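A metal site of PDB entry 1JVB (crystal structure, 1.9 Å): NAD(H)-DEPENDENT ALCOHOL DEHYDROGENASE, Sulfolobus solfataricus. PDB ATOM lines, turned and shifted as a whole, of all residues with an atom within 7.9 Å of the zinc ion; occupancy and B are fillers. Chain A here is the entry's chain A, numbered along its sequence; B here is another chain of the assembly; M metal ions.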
ATOM      1  N   GLN A  96     -18.215 -17.308   8.128  1.00  0.00           N
ATOM      2  CA  GLN A  96     -17.072 -18.226   7.975  1.00  0.00           C
ATOM      3  C   GLN A  96     -16.227 -18.066   6.745  1.00  0.00           C
ATOM      4  O   GLN A  96     -16.703 -17.637   5.690  1.00  0.00           O
ATOM      5  CB  GLN A  96     -17.612 -19.677   8.063  1.00  0.00           C
ATOM      6  CG  GLN A  96     -18.400 -19.870   9.326  1.00  0.00           C
ATOM      7  CD  GLN A  96     -18.928 -21.331   9.503  1.00  0.00           C
ATOM      8  OE1 GLN A  96     -18.521 -22.240   8.744  1.00  0.00           O
ATOM      9  NE2 GLN A  96     -19.782 -21.533  10.495  1.00  0.00           N
ATOM     10  N   GLY A  97     -14.937 -18.392   6.882  1.00  0.00           N
ATOM     11  CA  GLY A  97     -14.018 -18.235   5.767  1.00  0.00           C
ATOM     12  C   GLY A  97     -13.467 -19.615   5.400  1.00  0.00           C
ATOM     13  O   GLY A  97     -13.785 -20.601   6.039  1.00  0.00           O
ATOM     14  N   GLU A  98     -12.647 -19.680   4.363  1.00  0.00           N
ATOM     15  CA  GLU A  98     -12.112 -20.964   3.875  1.00  0.00           C
ATOM     16  C   GLU A  98     -10.678 -21.214   4.327  1.00  0.00           C
ATOM     17  O   GLU A  98     -10.217 -22.349   4.274  1.00  0.00           O
ATOM     18  CB  GLU A  98     -12.211 -20.970   2.357  1.00  0.00           C
ATOM     19  CG  GLU A  98     -11.853 -19.666   1.697  1.00  0.00           C
ATOM     20  CD  GLU A  98     -10.348 -19.391   1.700  1.00  0.00           C
ATOM     21  OE1 GLU A  98      -9.599 -20.311   1.284  1.00  0.00           O
ATOM     22  OE2 GLU A  98      -9.896 -18.248   2.018  1.00  0.00           O
ATOM     23  N   GLY A  99      -9.948 -20.162   4.730  1.00  0.00           N
ATOM     24  CA  GLY A  99      -8.614 -20.406   5.266  1.00  0.00           C
ATOM     25  C   GLY A  99      -7.389 -19.956   4.490  1.00  0.00           C
ATOM     26  O   GLY A  99      -6.405 -19.509   5.088  1.00  0.00           O
ATOM     27  N   ASN A 100      -7.442 -20.048   3.159  1.00  0.00           N
ATOM     28  CA  ASN A 100      -6.281 -19.753   2.306  1.00  0.00           C
ATOM     29  C   ASN A 100      -6.048 -18.295   1.916  1.00  0.00           C
ATOM     30  O   ASN A 100      -4.909 -17.925   1.690  1.00  0.00           O
ATOM     31  CB  ASN A 100      -6.406 -20.613   1.022  1.00  0.00           C
ATOM     32  CG  ASN A 100      -5.181 -20.609   0.158  1.00  0.00           C
ATOM     33  OD1 ASN A 100      -4.068 -20.917   0.609  1.00  0.00           O
ATOM     34  ND2 ASN A 100      -5.381 -20.303  -1.117  1.00  0.00           N
ATOM     35  N   CYS A 101      -7.106 -17.478   1.799  1.00  0.00           N
ATOM     36  CA  CYS A 101      -6.916 -16.100   1.312  1.00  0.00           C
ATOM     37  C   CYS A 101      -6.249 -15.225   2.379  1.00  0.00           C
ATOM     38  O   CYS A 101      -6.106 -15.611   3.528  1.00  0.00           O
ATOM     39  CB  CYS A 101      -8.252 -15.440   0.876  1.00  0.00           C
ATOM     40  SG  CYS A 101      -9.324 -14.930   2.291  1.00  0.00           S
ATOM     41  N   TYR A 102      -5.806 -14.081   1.916  1.00  0.00           N
ATOM     42  CA  TYR A 102      -5.145 -13.072   2.783  1.00  0.00           C
ATOM     43  C   TYR A 102      -5.913 -12.797   4.066  1.00  0.00           C
ATOM     44  O   TYR A 102      -5.376 -12.890   5.171  1.00  0.00           O
ATOM     45  CB  TYR A 102      -4.977 -11.796   1.982  1.00  0.00           C
ATOM     46  CG  TYR A 102      -4.463 -10.649   2.854  1.00  0.00           C
ATOM     47  CD1 TYR A 102      -3.087 -10.457   3.086  1.00  0.00           C
ATOM     48  CD2 TYR A 102      -5.371  -9.809   3.496  1.00  0.00           C
ATOM     49  CE1 TYR A 102      -2.641  -9.430   3.953  1.00  0.00           C
ATOM     50  CE2 TYR A 102      -4.936  -8.787   4.349  1.00  0.00           C
ATOM     51  CZ  TYR A 102      -3.589  -8.601   4.580  1.00  0.00           C
ATOM     52  OH  TYR A 102      -3.260  -7.567   5.450  1.00  0.00           O
ATOM     53  N   TYR A 103      -7.192 -12.490   3.927  1.00  0.00           N
ATOM     54  CA  TYR A 103      -8.027 -12.189   5.105  1.00  0.00           C
ATOM     55  C   TYR A 103      -8.136 -13.303   6.069  1.00  0.00           C
ATOM     56  O   TYR A 103      -8.126 -13.089   7.278  1.00  0.00           O
ATOM     57  CB  TYR A 103      -9.380 -11.669   4.615  1.00  0.00           C
ATOM     58  CG  TYR A 103      -9.169 -10.398   3.848  1.00  0.00           C
ATOM     59  CD1 TYR A 103      -8.924  -9.172   4.522  1.00  0.00           C
ATOM     60  CD2 TYR A 103      -9.049 -10.411   2.473  1.00  0.00           C
ATOM     61  CE1 TYR A 103      -8.562  -8.038   3.801  1.00  0.00           C
ATOM     62  CE2 TYR A 103      -8.687  -9.276   1.752  1.00  0.00           C
ATOM     63  CZ  TYR A 103      -8.441  -8.089   2.441  1.00  0.00           C
ATOM     64  OH  TYR A 103      -8.061  -7.004   1.709  1.00  0.00           O
ATOM     65  N   CYS A 104      -8.297 -14.553   5.594  1.00  0.00           N
ATOM     66  CA  CYS A 104      -8.328 -15.655   6.539  1.00  0.00           C
ATOM     67  C   CYS A 104      -6.979 -15.808   7.291  1.00  0.00           C
ATOM     68  O   CYS A 104      -6.958 -16.081   8.502  1.00  0.00           O
ATOM     69  CB  CYS A 104      -8.703 -16.972   5.806  1.00  0.00           C
ATOM     70  SG  CYS A 104     -10.478 -16.962   5.248  1.00  0.00           S
ATOM     71  N   ARG A 105      -5.861 -15.739   6.550  1.00  0.00           N
ATOM     72  CA  ARG A 105      -4.544 -15.914   7.130  1.00  0.00           C
ATOM     73  C   ARG A 105      -4.266 -14.891   8.243  1.00  0.00           C
ATOM     74  O   ARG A 105      -3.604 -15.227   9.210  1.00  0.00           O
ATOM     75  CB  ARG A 105      -3.484 -15.739   6.053  1.00  0.00           C
ATOM     76  CG  ARG A 105      -3.445 -16.990   5.125  1.00  0.00           C
ATOM     77  CD  ARG A 105      -2.332 -16.903   4.077  1.00  0.00           C
ATOM     78  NE  ARG A 105      -2.471 -17.980   3.058  1.00  0.00           N
ATOM     79  CZ  ARG A 105      -1.485 -18.796   2.656  1.00  0.00           C
ATOM     80  NH1 ARG A 105      -0.250 -18.716   3.194  1.00  0.00           N
ATOM     81  NH2 ARG A 105      -1.703 -19.638   1.599  1.00  0.00           N
ATOM     82  N   GLU A 108      -9.096 -12.321   9.873  1.00  0.00           N
ATOM     83  CA  GLU A 108     -10.293 -11.504   9.599  1.00  0.00           C
ATOM     84  C   GLU A 108     -11.157 -12.363   8.657  1.00  0.00           C
ATOM     85  O   GLU A 108     -11.450 -11.934   7.567  1.00  0.00           O
ATOM     86  CB  GLU A 108      -9.875 -10.223   8.869  1.00  0.00           C
ATOM     87  CG  GLU A 108      -8.833  -9.377   9.620  1.00  0.00           C
ATOM     88  CD  GLU A 108      -9.424  -8.710  10.857  1.00  0.00           C
ATOM     89  OE1 GLU A 108     -10.644  -8.621  10.960  1.00  0.00           O
ATOM     90  OE2 GLU A 108      -8.666  -8.281  11.743  1.00  0.00           O
ATOM     91  N   GLU A 109     -11.574 -13.529   9.134  1.00  0.00           N
ATOM     92  CA  GLU A 109     -12.291 -14.528   8.325  1.00  0.00           C
ATOM     93  C   GLU A 109     -13.593 -14.020   7.726  1.00  0.00           C
ATOM     94  O   GLU A 109     -14.028 -14.471   6.663  1.00  0.00           O
ATOM     95  CB  GLU A 109     -12.566 -15.785   9.172  1.00  0.00           C
ATOM     96  N   HIS A 110     -14.201 -13.026   8.350  1.00  0.00           N
ATOM     97  CA  HIS A 110     -15.458 -12.571   7.802  1.00  0.00           C
ATOM     98  C   HIS A 110     -15.289 -11.828   6.503  1.00  0.00           C
ATOM     99  O   HIS A 110     -16.264 -11.638   5.798  1.00  0.00           O
ATOM    100  CB  HIS A 110     -16.176 -11.719   8.855  1.00  0.00           C
ATOM    101  CG  HIS A 110     -15.446 -10.459   9.204  1.00  0.00           C
ATOM    102  ND1 HIS A 110     -14.186 -10.472   9.769  1.00  0.00           N
ATOM    103  CD2 HIS A 110     -15.806  -9.161   9.090  1.00  0.00           C
ATOM    104  CE1 HIS A 110     -13.802  -9.227   9.997  1.00  0.00           C
ATOM    105  NE2 HIS A 110     -14.775  -8.412   9.584  1.00  0.00           N
ATOM    106  N   LEU A 111     -14.043 -11.370   6.189  1.00  0.00           N
ATOM    107  CA  LEU A 111     -13.758 -10.647   4.977  1.00  0.00           C
ATOM    108  C   LEU A 111     -13.136 -11.552   3.917  1.00  0.00           C
ATOM    109  O   LEU A 111     -12.549 -11.093   2.933  1.00  0.00           O
ATOM    110  CB  LEU A 111     -12.791  -9.455   5.214  1.00  0.00           C
ATOM    111  CG  LEU A 111     -13.480  -8.446   6.139  1.00  0.00           C
ATOM    112  CD1 LEU A 111     -12.471  -7.334   6.496  1.00  0.00           C
ATOM    113  CD2 LEU A 111     -14.740  -7.884   5.454  1.00  0.00           C
ATOM    114  N   CYS A 112     -13.306 -12.841   4.158  1.00  0.00           N
ATOM    115  CA  CYS A 112     -12.814 -13.874   3.220  1.00  0.00           C
ATOM    116  C   CYS A 112     -13.179 -13.607   1.772  1.00  0.00           C
ATOM    117  O   CYS A 112     -14.287 -13.083   1.454  1.00  0.00           O
ATOM    118  CB  CYS A 112     -13.368 -15.206   3.688  1.00  0.00           C
ATOM    119  SG  CYS A 112     -12.931 -16.622   2.617  1.00  0.00           S
ATOM    120  N   ASP A 113     -12.255 -13.907   0.861  1.00  0.00           N
ATOM    121  CA  ASP A 113     -12.526 -13.709  -0.559  1.00  0.00           C
ATOM    122  C   ASP A 113     -13.614 -14.682  -1.123  1.00  0.00           C
ATOM    123  O   ASP A 113     -14.196 -14.398  -2.166  1.00  0.00           O
ATOM    124  CB  ASP A 113     -11.255 -13.926  -1.376  1.00  0.00           C
ATOM    125  CG  ASP A 113     -10.211 -12.852  -1.132  1.00  0.00           C
ATOM    126  OD1 ASP A 113     -10.573 -11.767  -0.620  1.00  0.00           O
ATOM    127  OD2 ASP A 113      -9.036 -13.117  -1.486  1.00  0.00           O
ATOM    128  N   SER A 114     -13.841 -15.793  -0.474  1.00  0.00           N
ATOM    129  CA  SER A 114     -14.844 -16.809  -0.928  1.00  0.00           C
ATOM    130  C   SER A 114     -15.589 -17.163   0.319  1.00  0.00           C
ATOM    131  O   SER A 114     -15.498 -18.275   0.843  1.00  0.00           O
ATOM    132  CB  SER A 114     -14.102 -18.032  -1.483  1.00  0.00           C
ATOM    133  OG  SER A 114     -13.242 -17.620  -2.521  1.00  0.00           O
ATOM    134  N   PRO A 115     -16.355 -16.189   0.854  1.00  0.00           N
ATOM    135  CA  PRO A 115     -17.076 -16.448   2.085  1.00  0.00           C
ATOM    136  C   PRO A 115     -18.065 -17.617   2.080  1.00  0.00           C
ATOM    137  O   PRO A 115     -18.635 -17.922   1.049  1.00  0.00           O
ATOM    138  CB  PRO A 115     -17.776 -15.130   2.357  1.00  0.00           C
ATOM    139  CG  PRO A 115     -18.080 -14.595   0.986  1.00  0.00           C
ATOM    140  CD  PRO A 115     -16.797 -14.964   0.177  1.00  0.00           C
ATOM    141  N   ARG A 116     -18.253 -18.182   3.256  1.00  0.00           N
ATOM    142  CA  ARG A 116     -19.216 -19.243   3.587  1.00  0.00           C
ATOM    143  C   ARG A 116     -20.087 -18.625   4.673  1.00  0.00           C
ATOM    144  O   ARG A 116     -19.886 -18.879   5.844  1.00  0.00           O
ATOM    145  CB  ARG A 116     -18.506 -20.417   4.191  1.00  0.00           C
ATOM    146  CG  ARG A 116     -17.675 -21.126   3.162  1.00  0.00           C
ATOM    147  CD  ARG A 116     -16.908 -22.191   3.880  1.00  0.00           C
ATOM    148  NE  ARG A 116     -15.944 -22.847   3.019  1.00  0.00           N
ATOM    149  CZ  ARG A 116     -15.156 -23.844   3.444  1.00  0.00           C
ATOM    150  NH1 ARG A 116     -15.222 -24.290   4.716  1.00  0.00           N
ATOM    151  NH2 ARG A 116     -14.294 -24.370   2.607  1.00  0.00           N
ATOM    152  N   LYS B 263     -10.050  -4.667   0.671  1.00  0.00           N
ATOM    153  CA  LYS B 263     -10.875  -4.677   1.853  1.00  0.00           C
ATOM    154  C   LYS B 263      -9.910  -4.320   3.030  1.00  0.00           C
ATOM    155  O   LYS B 263      -8.755  -4.811   3.115  1.00  0.00           O
ATOM    156  CB  LYS B 263     -11.509  -6.056   2.077  1.00  0.00           C
ATOM    157  CG  LYS B 263     -12.576  -6.362   0.997  1.00  0.00           C
ATOM    158  CD  LYS B 263     -13.073  -7.837   1.028  1.00  0.00           C
ATOM    159  CE  LYS B 263     -12.068  -8.785   0.371  1.00  0.00           C
ATOM    160  NZ  LYS B 263     -12.550 -10.187   0.541  1.00  0.00           N
HETATM  161 ZN    ZN M   1     -10.647 -16.647   3.042  1.00  0.00          ZN
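The zinc ion is bound by the side-chain carboxylate (OE2) of Glu 98 (2.0 Å), the side-chain sulfur (SG) of Cys 104 (2.2 Å), the side-chain sulfur (SG) of Cys 101 (2.3 Å) and the side-chain sulfur (SG) of Cys 112 (2.3 Å).
The side-chain amino group of Lys 263 of chain B lies within hydrogen-bond range of the backbone carbonyl oxygen of Cys 112, at 3.5 Å.
N of Gly 99 sits close to SG of Cys 104, at 3.3 Å.
N of Ser 114 sits close to SG of Cys 112.
OE1 of Glu 98 sits at hydrogen-bond distance from N of Asn 100 (2.9 Å).
OD1 of Asp 113 lies within salt-bridge range of NZ of Lys 263 of chain B (2.8 Å).
SG of Cys 101 sits close to N of Tyr 103, 3.6 Å away.
The backbone NH (N) of Asp 113 sits close to the side-chain sulfur (SG) of Cys 101 (3.4 Å).
Merely in contact with the zinc ion: Asp 113 and Gly 99.
Six residues have an atom within 4 Å of the zinc ion: Glu 98, Gly 99, Cys 101, Cys 104, Cys 112 and Asp 113.
The nearest printed residue that does not touch the zinc ion is Gly 97 (4.6 Å).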
